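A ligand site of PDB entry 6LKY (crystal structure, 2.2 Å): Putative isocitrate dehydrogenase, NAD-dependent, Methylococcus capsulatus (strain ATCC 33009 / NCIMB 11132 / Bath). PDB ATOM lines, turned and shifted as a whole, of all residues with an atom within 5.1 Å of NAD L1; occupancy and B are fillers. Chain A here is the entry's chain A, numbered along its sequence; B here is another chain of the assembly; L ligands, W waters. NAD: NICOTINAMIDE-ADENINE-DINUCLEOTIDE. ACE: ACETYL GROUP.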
ATOM      1  N   ILE A  12      -8.514   2.853   4.882  1.00  0.00           N
ATOM      2  CA  ILE A  12      -7.936   2.039   3.815  1.00  0.00           C
ATOM      3  C   ILE A  12      -6.987   2.830   2.921  1.00  0.00           C
ATOM      4  O   ILE A  12      -6.335   2.229   2.056  1.00  0.00           O
ATOM      5  CB  ILE A  12      -9.053   1.395   2.957  1.00  0.00           C
ATOM      6  CG1 ILE A  12      -9.974   2.466   2.379  1.00  0.00           C
ATOM      7  CG2 ILE A  12      -9.829   0.365   3.797  1.00  0.00           C
ATOM      8  CD1 ILE A  12     -10.831   1.966   1.233  1.00  0.00           C
ATOM      9  N   LYS A  66      -3.957  11.807  -3.670  1.00  0.00           N
ATOM     10  CA  LYS A  66      -4.522  11.905  -2.319  1.00  0.00           C
ATOM     11  C   LYS A  66      -5.414  10.712  -2.019  1.00  0.00           C
ATOM     12  O   LYS A  66      -6.404  10.471  -2.716  1.00  0.00           O
ATOM     13  CB  LYS A  66      -5.320  13.210  -2.152  1.00  0.00           C
ATOM     14  CG  LYS A  66      -5.781  13.456  -0.713  1.00  0.00           C
ATOM     15  CD  LYS A  66      -6.963  14.448  -0.637  1.00  0.00           C
ATOM     16  CE  LYS A  66      -8.153  14.000  -1.461  1.00  0.00           C
ATOM     17  NZ  LYS A  66      -8.883  12.814  -0.910  1.00  0.00           N
ATOM     18  N   GLY A  67      -5.060   9.956  -0.991  1.00  0.00           N
ATOM     19  CA  GLY A  67      -5.930   8.917  -0.474  1.00  0.00           C
ATOM     20  C   GLY A  67      -7.135   9.531   0.216  1.00  0.00           C
ATOM     21  O   GLY A  67      -7.197  10.744   0.435  1.00  0.00           O
ATOM     22  N   PRO A  68      -8.121   8.711   0.582  1.00  0.00           N
ATOM     23  CA  PRO A  68      -9.331   9.242   1.218  1.00  0.00           C
ATOM     24  C   PRO A  68      -9.032   9.858   2.570  1.00  0.00           C
ATOM     25  O   PRO A  68      -8.199   9.353   3.322  1.00  0.00           O
ATOM     26  CB  PRO A  68     -10.227   8.011   1.355  1.00  0.00           C
ATOM     27  CG  PRO A  68      -9.234   6.846   1.421  1.00  0.00           C
ATOM     28  CD  PRO A  68      -8.170   7.245   0.428  1.00  0.00           C
ATOM     29  N   LEU A  69      -9.711  10.962   2.873  1.00  0.00           N
ATOM     30  CA  LEU A  69      -9.514  11.661   4.135  1.00  0.00           C
ATOM     31  C   LEU A  69     -10.806  11.606   4.937  1.00  0.00           C
ATOM     32  O   LEU A  69     -11.884  11.931   4.415  1.00  0.00           O
ATOM     33  CB  LEU A  69      -9.082  13.103   3.884  1.00  0.00           C
ATOM     34  CG  LEU A  69      -7.711  13.203   3.194  1.00  0.00           C
ATOM     35  CD1 LEU A  69      -7.270  14.656   3.006  1.00  0.00           C
ATOM     36  CD2 LEU A  69      -6.676  12.421   3.997  1.00  0.00           C
ATOM     37  N   THR A  70     -10.705  11.172   6.198  1.00  0.00           N
ATOM     38  CA  THR A  70     -11.870  11.135   7.092  1.00  0.00           C
ATOM     39  C   THR A  70     -12.340  12.549   7.437  1.00  0.00           C
ATOM     40  O   THR A  70     -11.535  13.405   7.793  1.00  0.00           O
ATOM     41  CB  THR A  70     -11.486  10.377   8.370  1.00  0.00           C
ATOM     42  OG1 THR A  70     -11.384   8.982   8.077  1.00  0.00           O
ATOM     43  CG2 THR A  70     -12.526  10.618   9.505  1.00  0.00           C
ATOM     44  N   THR A  71     -13.657  12.788   7.347  1.00  0.00           N
ATOM     45  CA  THR A  71     -14.252  14.002   7.874  1.00  0.00           C
ATOM     46  C   THR A  71     -15.227  13.654   8.988  1.00  0.00           C
ATOM     47  O   THR A  71     -16.136  12.848   8.768  1.00  0.00           O
ATOM     48  CB  THR A  71     -14.983  14.787   6.756  1.00  0.00           C
ATOM     49  OG1 THR A  71     -14.052  15.111   5.717  1.00  0.00           O
ATOM     50  CG2 THR A  71     -15.627  16.086   7.305  1.00  0.00           C
ATOM     51  N   PRO A  72     -15.094  14.247  10.182  1.00  0.00           N
ATOM     52  CA  PRO A  72     -16.034  13.932  11.271  1.00  0.00           C
ATOM     53  C   PRO A  72     -17.433  14.457  11.007  1.00  0.00           C
ATOM     54  O   PRO A  72     -17.632  15.494  10.357  1.00  0.00           O
ATOM     55  CB  PRO A  72     -15.409  14.590  12.508  1.00  0.00           C
ATOM     56  CG  PRO A  72     -14.090  15.191  12.062  1.00  0.00           C
ATOM     57  CD  PRO A  72     -14.082  15.237  10.570  1.00  0.00           C
ATOM     58  N   ASN A  81     -10.791  17.503   2.379  1.00  0.00           N
ATOM     59  CA  ASN A  81     -10.982  17.382   0.935  1.00  0.00           C
ATOM     60  C   ASN A  81     -11.517  18.687   0.361  1.00  0.00           C
ATOM     61  O   ASN A  81     -11.002  19.211  -0.634  1.00  0.00           O
ATOM     62  CB  ASN A  81     -11.920  16.225   0.631  1.00  0.00           C
ATOM     63  CG  ASN A  81     -11.417  14.916   1.220  1.00  0.00           C
ATOM     64  OD1 ASN A  81     -10.328  14.460   0.890  1.00  0.00           O
ATOM     65  ND2 ASN A  81     -12.200  14.324   2.137  1.00  0.00           N
ATOM     66  N   ARG A  85      -9.725  21.504  -2.100  1.00  0.00           N
ATOM     67  CA  ARG A  85     -10.346  21.921  -3.361  1.00  0.00           C
ATOM     68  C   ARG A  85     -10.499  23.438  -3.429  1.00  0.00           C
ATOM     69  O   ARG A  85     -10.241  24.058  -4.470  1.00  0.00           O
ATOM     70  CB  ARG A  85     -11.726  21.264  -3.534  1.00  0.00           C
ATOM     71  CG  ARG A  85     -11.700  19.772  -3.717  1.00  0.00           C
ATOM     72  CD  ARG A  85     -13.027  19.128  -3.360  1.00  0.00           C
ATOM     73  NE  ARG A  85     -12.951  17.679  -3.567  1.00  0.00           N
ATOM     74  CZ  ARG A  85     -13.811  16.798  -3.071  1.00  0.00           C
ATOM     75  NH1 ARG A  85     -14.833  17.217  -2.328  1.00  0.00           N
ATOM     76  NH2 ARG A  85     -13.650  15.507  -3.313  1.00  0.00           N
ATOM     77  N   ARG A  95     -15.519  13.017 -12.854  1.00  0.00           N
ATOM     78  CA  ARG A  95     -15.700  11.642 -12.395  1.00  0.00           C
ATOM     79  C   ARG A  95     -16.263  10.755 -13.496  1.00  0.00           C
ATOM     80  O   ARG A  95     -17.493  10.746 -13.712  1.00  0.00           O
ATOM     81  CB  ARG A  95     -16.575  11.605 -11.157  1.00  0.00           C
ATOM     82  CG  ARG A  95     -15.875  12.212  -9.946  1.00  0.00           C
ATOM     83  CD  ARG A  95     -16.784  12.350  -8.750  1.00  0.00           C
ATOM     84  NE  ARG A  95     -16.001  12.716  -7.574  1.00  0.00           N
ATOM     85  CZ  ARG A  95     -16.404  12.521  -6.322  1.00  0.00           C
ATOM     86  NH1 ARG A  95     -17.605  12.007  -6.079  1.00  0.00           N
ATOM     87  NH2 ARG A  95     -15.610  12.871  -5.328  1.00  0.00           N
ATOM     88  N   LEU A 244     -17.970   1.728  -5.421  1.00  0.00           N
ATOM     89  CA  LEU A 244     -17.025   2.788  -5.108  1.00  0.00           C
ATOM     90  C   LEU A 244     -15.581   2.319  -5.187  1.00  0.00           C
ATOM     91  O   LEU A 244     -14.675   3.144  -5.359  1.00  0.00           O
ATOM     92  CB  LEU A 244     -17.278   3.313  -3.696  1.00  0.00           C
ATOM     93  CG  LEU A 244     -18.536   4.137  -3.442  1.00  0.00           C
ATOM     94  CD1 LEU A 244     -18.640   4.486  -1.965  1.00  0.00           C
ATOM     95  CD2 LEU A 244     -18.498   5.406  -4.289  1.00  0.00           C
ATOM     96  N   GLY A 245     -15.348   1.010  -5.031  1.00  0.00           N
ATOM     97  CA  GLY A 245     -14.007   0.462  -5.177  1.00  0.00           C
ATOM     98  C   GLY A 245     -13.409   0.656  -6.546  1.00  0.00           C
ATOM     99  O   GLY A 245     -12.203   0.418  -6.709  1.00  0.00           O
ATOM    100  N   GLU A 260      -7.823  11.498  -6.960  1.00  0.00           N
ATOM    101  CA  GLU A 260      -8.218  10.714  -5.805  1.00  0.00           C
ATOM    102  C   GLU A 260      -9.255   9.666  -6.186  1.00  0.00           C
ATOM    103  O   GLU A 260      -9.898   9.762  -7.229  1.00  0.00           O
ATOM    104  CB  GLU A 260      -8.808  11.629  -4.710  1.00  0.00           C
ATOM    105  CG  GLU A 260     -10.082  12.348  -5.184  1.00  0.00           C
ATOM    106  CD  GLU A 260     -10.728  13.236  -4.114  1.00  0.00           C
ATOM    107  OE1 GLU A 260     -10.545  12.959  -2.904  1.00  0.00           O
ATOM    108  OE2 GLU A 260     -11.421  14.216  -4.483  1.00  0.00           O
ATOM    109  N   ALA A 261      -9.416   8.670  -5.314  1.00  0.00           N
ATOM    110  CA  ALA A 261     -10.597   7.833  -5.405  1.00  0.00           C
ATOM    111  C   ALA A 261     -11.844   8.622  -5.005  1.00  0.00           C
ATOM    112  O   ALA A 261     -11.777   9.629  -4.286  1.00  0.00           O
ATOM    113  CB  ALA A 261     -10.445   6.575  -4.531  1.00  0.00           C
ATOM    114  N   VAL A 262     -12.984   8.163  -5.506  1.00  0.00           N
ATOM    115  CA  VAL A 262     -14.267   8.754  -5.134  1.00  0.00           C
ATOM    116  C   VAL A 262     -14.683   8.347  -3.722  1.00  0.00           C
ATOM    117  O   VAL A 262     -15.349   9.116  -3.017  1.00  0.00           O
ATOM    118  CB  VAL A 262     -15.312   8.354  -6.201  1.00  0.00           C
ATOM    119  CG1 VAL A 262     -16.725   8.487  -5.658  1.00  0.00           C
ATOM    120  CG2 VAL A 262     -15.100   9.162  -7.491  1.00  0.00           C
ATOM    121  N   HIS A 263     -14.280   7.159  -3.295  1.00  0.00           N
ATOM    122  CA  HIS A 263     -14.763   6.608  -2.047  1.00  0.00           C
ATOM    123  C   HIS A 263     -14.049   7.250  -0.861  1.00  0.00           C
ATOM    124  O   HIS A 263     -13.094   8.030  -1.022  1.00  0.00           O
ATOM    125  CB  HIS A 263     -14.588   5.084  -2.031  1.00  0.00           C
ATOM    126  CG  HIS A 263     -13.161   4.622  -2.119  1.00  0.00           C
ATOM    127  ND1 HIS A 263     -12.232   4.857  -1.129  1.00  0.00           N
ATOM    128  CD2 HIS A 263     -12.521   3.900  -3.075  1.00  0.00           C
ATOM    129  CE1 HIS A 263     -11.079   4.326  -1.479  1.00  0.00           C
ATOM    130  NE2 HIS A 263     -11.229   3.736  -2.657  1.00  0.00           N
ATOM    131  N   GLY A 264     -14.511   6.918   0.338  1.00  0.00           N
ATOM    132  CA  GLY A 264     -13.932   7.403   1.566  1.00  0.00           C
ATOM    133  C   GLY A 264     -12.945   6.446   2.215  1.00  0.00           C
ATOM    134  O   GLY A 264     -12.380   5.548   1.575  1.00  0.00           O
ATOM    135  N   SER A 265     -12.704   6.666   3.508  1.00  0.00           N
ATOM    136  CA  SER A 265     -11.692   5.908   4.230  1.00  0.00           C
ATOM    137  C   SER A 265     -12.184   4.526   4.675  1.00  0.00           C
ATOM    138  O   SER A 265     -11.402   3.785   5.282  1.00  0.00           O
ATOM    139  CB  SER A 265     -11.204   6.705   5.445  1.00  0.00           C
ATOM    140  OG  SER A 265     -12.289   7.200   6.209  1.00  0.00           O
ATOM    141  N   ALA A 266     -13.446   4.186   4.422  1.00  0.00           N
ATOM    142  CA  ALA A 266     -14.028   2.858   4.680  1.00  0.00           C
ATOM    143  C   ALA A 266     -13.610   2.295   6.035  1.00  0.00           C
ATOM    144  O   ALA A 266     -12.910   1.277   6.094  1.00  0.00           O
ATOM    145  CB  ALA A 266     -13.635   1.901   3.552  1.00  0.00           C
ATOM    146  N   PRO A 267     -14.036   2.911   7.145  1.00  0.00           N
ATOM    147  CA  PRO A 267     -13.616   2.393   8.458  1.00  0.00           C
ATOM    148  C   PRO A 267     -14.100   0.975   8.737  1.00  0.00           C
ATOM    149  O   PRO A 267     -13.483   0.284   9.556  1.00  0.00           O
ATOM    150  CB  PRO A 267     -14.207   3.406   9.458  1.00  0.00           C
ATOM    151  CG  PRO A 267     -15.300   4.114   8.697  1.00  0.00           C
ATOM    152  CD  PRO A 267     -14.874   4.124   7.256  1.00  0.00           C
ATOM    153  N   ASP A 268     -15.187   0.525   8.108  1.00  0.00           N
ATOM    154  CA  ASP A 268     -15.676  -0.820   8.380  1.00  0.00           C
ATOM    155  C   ASP A 268     -14.704  -1.910   7.913  1.00  0.00           C
ATOM    156  O   ASP A 268     -14.773  -3.038   8.422  1.00  0.00           O
ATOM    157  CB  ASP A 268     -17.068  -1.056   7.770  1.00  0.00           C
ATOM    158  CG  ASP A 268     -17.130  -0.719   6.282  1.00  0.00           C
ATOM    159  OD1 ASP A 268     -16.240  -0.013   5.786  1.00  0.00           O
ATOM    160  OD2 ASP A 268     -18.081  -1.172   5.611  1.00  0.00           O
ATOM    161  N   ILE A 269     -13.815  -1.619   6.961  1.00  0.00           N
ATOM    162  CA  ILE A 269     -12.853  -2.596   6.478  1.00  0.00           C
ATOM    163  C   ILE A 269     -11.419  -2.112   6.604  1.00  0.00           C
ATOM    164  O   ILE A 269     -10.506  -2.738   6.051  1.00  0.00           O
ATOM    165  CB  ILE A 269     -13.153  -3.005   5.019  1.00  0.00           C
ATOM    166  CG1 ILE A 269     -13.027  -1.817   4.074  1.00  0.00           C
ATOM    167  CG2 ILE A 269     -14.525  -3.661   4.903  1.00  0.00           C
ATOM    168  CD1 ILE A 269     -12.986  -2.199   2.605  1.00  0.00           C
ATOM    169  N   ILE A 274      -8.563  -5.910   2.572  1.00  0.00           N
ATOM    170  CA  ILE A 274      -9.440  -6.411   1.515  1.00  0.00           C
ATOM    171  C   ILE A 274      -9.982  -5.312   0.606  1.00  0.00           C
ATOM    172  O   ILE A 274     -10.695  -5.620  -0.354  1.00  0.00           O
ATOM    173  CB  ILE A 274     -10.606  -7.234   2.109  1.00  0.00           C
ATOM    174  CG1 ILE A 274     -11.472  -6.361   3.017  1.00  0.00           C
ATOM    175  CG2 ILE A 274     -10.083  -8.447   2.874  1.00  0.00           C
ATOM    176  CD1 ILE A 274     -12.798  -6.997   3.404  1.00  0.00           C
ATOM    177  N   ALA A 275      -9.688  -4.040   0.880  1.00  0.00           N
ATOM    178  CA  ALA A 275     -10.192  -2.946   0.058  1.00  0.00           C
ATOM    179  C   ALA A 275      -9.779  -3.104  -1.408  1.00  0.00           C
ATOM    180  O   ALA A 275      -8.646  -3.448  -1.721  1.00  0.00           O
ATOM    181  CB  ALA A 275      -9.700  -1.593   0.589  1.00  0.00           C
ATOM    182  N   ASN A 276     -10.723  -2.805  -2.306  1.00  0.00           N
ATOM    183  CA  ASN A 276     -10.441  -2.763  -3.736  1.00  0.00           C
ATOM    184  C   ASN A 276      -9.542  -1.589  -4.066  1.00  0.00           C
ATOM    185  O   ASN A 276      -9.898  -0.444  -3.750  1.00  0.00           O
ATOM    186  CB  ASN A 276     -11.734  -2.672  -4.524  1.00  0.00           C
ATOM    187  CG  ASN A 276     -11.544  -2.966  -5.994  1.00  0.00           C
ATOM    188  OD1 ASN A 276     -10.437  -2.825  -6.542  1.00  0.00           O
ATOM    189  ND2 ASN A 276     -12.625  -3.377  -6.653  1.00  0.00           N
ATOM    190  N   ASP A 317     -15.277  -7.224  -2.814  1.00  0.00           N
ATOM    191  CA  ASP A 317     -16.359  -6.364  -3.289  1.00  0.00           C
ATOM    192  C   ASP A 317     -16.776  -6.724  -4.712  1.00  0.00           C
ATOM    193  O   ASP A 317     -17.936  -6.502  -5.093  1.00  0.00           O
ATOM    194  CB  ASP A 317     -15.954  -4.907  -3.228  1.00  0.00           C
ATOM    195  CG  ASP A 317     -14.734  -4.618  -4.069  1.00  0.00           C
ATOM    196  OD1 ASP A 317     -13.670  -5.185  -3.749  1.00  0.00           O
ATOM    197  OD2 ASP A 317     -14.836  -3.861  -5.060  1.00  0.00           O
ATOM    198  N   ASN B 176     -21.280  15.175   7.822  1.00  0.00           N
ATOM    199  CA  ASN B 176     -19.867  15.521   7.765  1.00  0.00           C
ATOM    200  C   ASN B 176     -19.656  16.890   7.143  1.00  0.00           C
ATOM    201  O   ASN B 176     -18.762  17.632   7.567  1.00  0.00           O
ATOM    202  CB  ASN B 176     -19.063  14.448   7.004  1.00  0.00           C
ATOM    203  CG  ASN B 176     -19.663  14.109   5.639  1.00  0.00           C
ATOM    204  OD1 ASN B 176     -20.802  14.450   5.329  1.00  0.00           O
ATOM    205  ND2 ASN B 176     -18.882  13.419   4.829  1.00  0.00           N
ATOM    206  N   ILE B 205     -24.354   8.225   5.306  1.00  0.00           N
ATOM    207  CA  ILE B 205     -24.155   9.451   4.530  1.00  0.00           C
ATOM    208  C   ILE B 205     -24.809   9.281   3.159  1.00  0.00           C
ATOM    209  O   ILE B 205     -24.690   8.220   2.524  1.00  0.00           O
ATOM    210  CB  ILE B 205     -22.655   9.771   4.440  1.00  0.00           C
ATOM    211  CG1 ILE B 205     -22.087   9.917   5.872  1.00  0.00           C
ATOM    212  CG2 ILE B 205     -22.408  11.064   3.637  1.00  0.00           C
ATOM    213  CD1 ILE B 205     -20.566  10.123   5.947  1.00  0.00           C
ATOM    214  N   ASP B 207     -24.494  10.044   0.063  1.00  0.00           N
ATOM    215  CA  ASP B 207     -23.885   9.588  -1.186  1.00  0.00           C
ATOM    216  C   ASP B 207     -23.555   8.086  -1.136  1.00  0.00           C
ATOM    217  O   ASP B 207     -23.895   7.335  -2.065  1.00  0.00           O
ATOM    218  CB  ASP B 207     -22.649  10.435  -1.543  1.00  0.00           C
ATOM    219  CG  ASP B 207     -21.590  10.486  -0.428  1.00  0.00           C
ATOM    220  OD1 ASP B 207     -21.828   9.925   0.667  1.00  0.00           O
ATOM    221  OD2 ASP B 207     -20.506  11.075  -0.661  1.00  0.00           O
ATOM    222  N   ALA B 208     -22.953   7.631  -0.034  1.00  0.00           N
ATOM    223  CA  ALA B 208     -22.745   6.187   0.144  1.00  0.00           C
ATOM    224  C   ALA B 208     -24.083   5.448   0.113  1.00  0.00           C
ATOM    225  O   ALA B 208     -24.185   4.358  -0.449  1.00  0.00           O
ATOM    226  CB  ALA B 208     -22.008   5.893   1.450  1.00  0.00           C
ATOM    227  N   MET B 211     -25.214   4.904  -3.485  1.00  0.00           N
ATOM    228  CA  MET B 211     -24.462   3.769  -4.039  1.00  0.00           C
ATOM    229  C   MET B 211     -25.030   2.445  -3.538  1.00  0.00           C
ATOM    230  O   MET B 211     -25.249   1.511  -4.322  1.00  0.00           O
ATOM    231  CB  MET B 211     -22.982   3.900  -3.692  1.00  0.00           C
ATOM    232  CG  MET B 211     -22.145   2.644  -3.978  1.00  0.00           C
ATOM    233  SD  MET B 211     -22.290   1.342  -2.714  1.00  0.00           S
ATOM    234  CE  MET B 211     -21.412   2.079  -1.312  1.00  0.00           C
ATOM    235  N   GLN B 212     -25.299   2.367  -2.233  1.00  0.00           N
ATOM    236  CA  GLN B 212     -25.802   1.123  -1.639  1.00  0.00           C
ATOM    237  C   GLN B 212     -27.194   0.779  -2.134  1.00  0.00           C
ATOM    238  O   GLN B 212     -27.520  -0.393  -2.315  1.00  0.00           O
ATOM    239  CB  GLN B 212     -25.800   1.217  -0.113  1.00  0.00           C
ATOM    240  CG  GLN B 212     -24.427   0.968   0.510  1.00  0.00           C
ATOM    241  CD  GLN B 212     -24.309   1.437   1.957  1.00  0.00           C
ATOM    242  OE1 GLN B 212     -25.302   1.658   2.637  1.00  0.00           O
ATOM    243  NE2 GLN B 212     -23.076   1.594   2.425  1.00  0.00           N
HETATM  244  PA  NAD L   1     -17.027   5.129   2.432  1.00  0.00           P
HETATM  245  O1A NAD L   1     -15.783   5.257   3.267  1.00  0.00           O
HETATM  246  O2A NAD L   1     -16.732   5.408   0.983  1.00  0.00           O
HETATM  247  O5B NAD L   1     -17.658   3.678   2.651  1.00  0.00           O
HETATM  248  C5B NAD L   1     -18.904   3.369   2.024  1.00  0.00           C
HETATM  249  C4B NAD L   1     -18.973   1.869   1.788  1.00  0.00           C
HETATM  250  O4B NAD L   1     -18.127   1.577   0.657  1.00  0.00           O
HETATM  251  C3B NAD L   1     -18.433   1.124   2.994  1.00  0.00           C
HETATM  252  O3B NAD L   1     -19.216  -0.032   3.267  1.00  0.00           O
HETATM  253  C2B NAD L   1     -17.026   0.743   2.572  1.00  0.00           C
HETATM  254  O2B NAD L   1     -16.529  -0.454   3.186  1.00  0.00           O
HETATM  255  C1B NAD L   1     -17.129   0.642   1.054  1.00  0.00           C
HETATM  256  N9A NAD L   1     -15.789   0.988   0.590  1.00  0.00           N
HETATM  257  C8A NAD L   1     -15.542   2.319   0.011  1.00  0.00           C
HETATM  258  N7A NAD L   1     -14.172   2.088  -0.491  1.00  0.00           N
HETATM  259  C5A NAD L   1     -14.313   0.849  -1.254  1.00  0.00           C
HETATM  260  C6A NAD L   1     -13.009   0.067  -1.279  1.00  0.00           C
HETATM  261  N6A NAD L   1     -12.064   0.747  -2.176  1.00  0.00           N
HETATM  262  N1A NAD L   1     -13.316  -1.275  -1.800  1.00  0.00           N
HETATM  263  C2A NAD L   1     -14.227  -2.065  -0.959  1.00  0.00           C
HETATM  264  N3A NAD L   1     -14.836  -1.244   0.104  1.00  0.00           N
HETATM  265  C4A NAD L   1     -15.284   0.047  -0.420  1.00  0.00           C
HETATM  266  O3  NAD L   1     -18.136   6.199   2.877  1.00  0.00           O
HETATM  267  PN  NAD L   1     -18.584   6.526   4.374  1.00  0.00           P
HETATM  268  O1N NAD L   1     -18.532   5.353   5.301  1.00  0.00           O
HETATM  269  O2N NAD L   1     -19.983   7.110   4.255  1.00  0.00           O
HETATM  270  O5D NAD L   1     -17.568   7.653   4.908  1.00  0.00           O
HETATM  271  C5D NAD L   1     -16.373   7.275   5.611  1.00  0.00           C
HETATM  272  C4D NAD L   1     -15.453   8.482   5.722  1.00  0.00           C
HETATM  273  O4D NAD L   1     -14.838   8.798   4.460  1.00  0.00           O
HETATM  274  C3D NAD L   1     -16.220   9.714   6.184  1.00  0.00           C
HETATM  275  O3D NAD L   1     -15.469  10.337   7.230  1.00  0.00           O
HETATM  276  C2D NAD L   1     -16.240  10.596   4.946  1.00  0.00           C
HETATM  277  O2D NAD L   1     -16.228  11.997   5.225  1.00  0.00           O
HETATM  278  C1D NAD L   1     -14.949  10.216   4.230  1.00  0.00           C
HETATM  279  N1N NAD L   1     -15.048  10.643   2.813  1.00  0.00           N
HETATM  280  C2N NAD L   1     -13.762  10.705   2.125  1.00  0.00           C
HETATM  281  C3N NAD L   1     -14.039  11.366   0.794  1.00  0.00           C
HETATM  282  C7N NAD L   1     -12.789  11.920   0.113  1.00  0.00           C
HETATM  283  O7N NAD L   1     -12.823  11.765  -1.296  1.00  0.00           O
HETATM  284  N7N NAD L   1     -11.569  11.386   0.718  1.00  0.00           N
HETATM  285  C4N NAD L   1     -14.932  10.543  -0.132  1.00  0.00           C
HETATM  286  C5N NAD L   1     -16.167  10.015   0.585  1.00  0.00           C
HETATM  287  C6N NAD L   1     -16.113   9.890   2.104  1.00  0.00           C
HETATM  288  C   ACE L   2     -18.050  -1.094  -2.618  1.00  0.00           C
HETATM  289  O   ACE L   2     -17.036  -0.839  -3.274  1.00  0.00           O
HETATM  290  CH3 ACE L   2     -19.310  -0.323  -2.814  1.00  0.00           C
HETATM  291  O   HOH W   1     -19.742   9.115   2.104  1.00  0.00           O
HETATM  292  O   HOH W   2     -18.749   7.457   0.093  1.00  0.00           O
HETATM  293  O   HOH W   3     -10.642   9.756  -1.644  1.00  0.00           O
HETATM  294  O   HOH W   4     -22.225   6.292   5.269  1.00  0.00           O
HETATM  295  O   HOH W   5     -13.148  -5.301  -1.031  1.00  0.00           O
HETATM  296  O   HOH W   6     -18.915   5.967   7.854  1.00  0.00           O
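Water W4 lies within hydrogen-bond range of an oxygen (O2N) of NAD L1 (2.6 Å) and the backbone NH of Ile 205 of chain B (2.9 Å). Water W1 bridges the side-chain carboxylate of Asp 207 of chain B (2.7 Å) and an oxygen (O2N) of NAD L1 (3.0 Å). Water W5 bridges the backbone carbonyl oxygen of Ile 274 (2.6 Å) and the side-chain carboxylate of Asp 317 (2.8 Å).
The side-chain amino group of Lys 66 lies close to a nitrogen (N7N) of NAD L1 (3.5 Å). The backbone NH (N) of Leu 69 lies close to a nitrogen (N7N) of NAD L1. The side-chain carboxylate (OE1) of Glu 260 lies close to an oxygen (O7N) of NAD L1, 3.0 Å away. Residues that only touch NAD L1: Ile 12 (3.8 Å), Pro 68 (3.1 Å), Thr 70 (3.7 Å), Leu 244 (3.6 Å), Gly 245 (3.6 Å), Ala 261 (3.8 Å), Val 262 (3.2 Å), Pro 267 (3.9 Å), Ile 269 (3.3 Å), Ile 205 of chain B (3.5 Å), Ala 208 of chain B (3.7 Å) and Met 211 of chain B (3.9 Å). The nearest printed residue that does not touch NAD L1 is Ala 275 (4.0005 Å).
The side-chain hydroxyl of Ser 265 sits at hydrogen-bond distance from the side-chain hydroxyl of Thr 70. The backbone carbonyl oxygen of Ser 265 lies within hydrogen-bond range of the backbone NH of Ile 12 (3.1 Å). The side-chain amide oxygen of Asn 81 lies within hydrogen-bond range of the side-chain amino group of Lys 66. The guanidinium group (NH2) of Arg 85 is in salt-bridge range of the side-chain carboxylate (OE2) of Glu 260 (2.8 Å). O of Leu 69 lies within hydrogen-bond range of ND2 of Asn 81. The side-chain amino group (NZ) of Lys 66 is in salt-bridge range of the side-chain carboxylate (OE1) of Glu 260 (2.6 Å). The side-chain amide nitrogen (ND2) of Asn 276 sits at hydrogen-bond distance from the side-chain carboxylate (OD2) of Asp 317 (2.8 Å).
The backbone NH (N) of Leu 244 sits at hydrogen-bond distance from an oxygen (O) of ACE L2 (3.5 Å). An oxygen (O3D) of NAD L1 lies within hydrogen-bond range of the backbone NH (N) of Thr 71, 3.1 Å away. The side-chain hydroxyl (OG) of Ser 265 lies close to an oxygen (O4D) of NAD L1. The backbone NH of Gly 245 lies within hydrogen-bond range of an oxygen (O) of ACE L2 (3.1 Å). The backbone NH (N) of Ser 265 sits at hydrogen-bond distance from an oxygen (O4D) of NAD L1 (3.2 Å). N of Asn 276 is in hydrogen-bond range of N1A of NAD L1 (3.1 Å). The side-chain amide oxygen (OD1) of Asn 81 lies within hydrogen-bond range of a nitrogen (N7N) of NAD L1. The side-chain amide nitrogen of Asn 176 of chain B is in hydrogen-bond range of an oxygen (O2D) of NAD L1 (3.0 Å). A ring nitrogen (NE2) of His 263 sits at hydrogen-bond distance from a nitrogen (N6A) of NAD L1 (3.1 Å). O1A of NAD L1 sits at hydrogen-bond distance from N of Ala 266, 2.8 Å away. An oxygen (O2B) of NAD L1 is in hydrogen-bond range of the side-chain carboxylate (OD1) of Asp 268 (2.7 Å). The backbone carbonyl oxygen (O) of Asn 276 is in hydrogen-bond range of a nitrogen (N6A) of NAD L1, 2.9 Å away. The backbone NH (N) of Gly 264 lies within hydrogen-bond range of an oxygen (O2A) of NAD L1 (2.8 Å). The backbone carbonyl oxygen of Thr 71 is in hydrogen-bond range of an oxygen (O3D) of NAD L1, 3.0 Å away.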
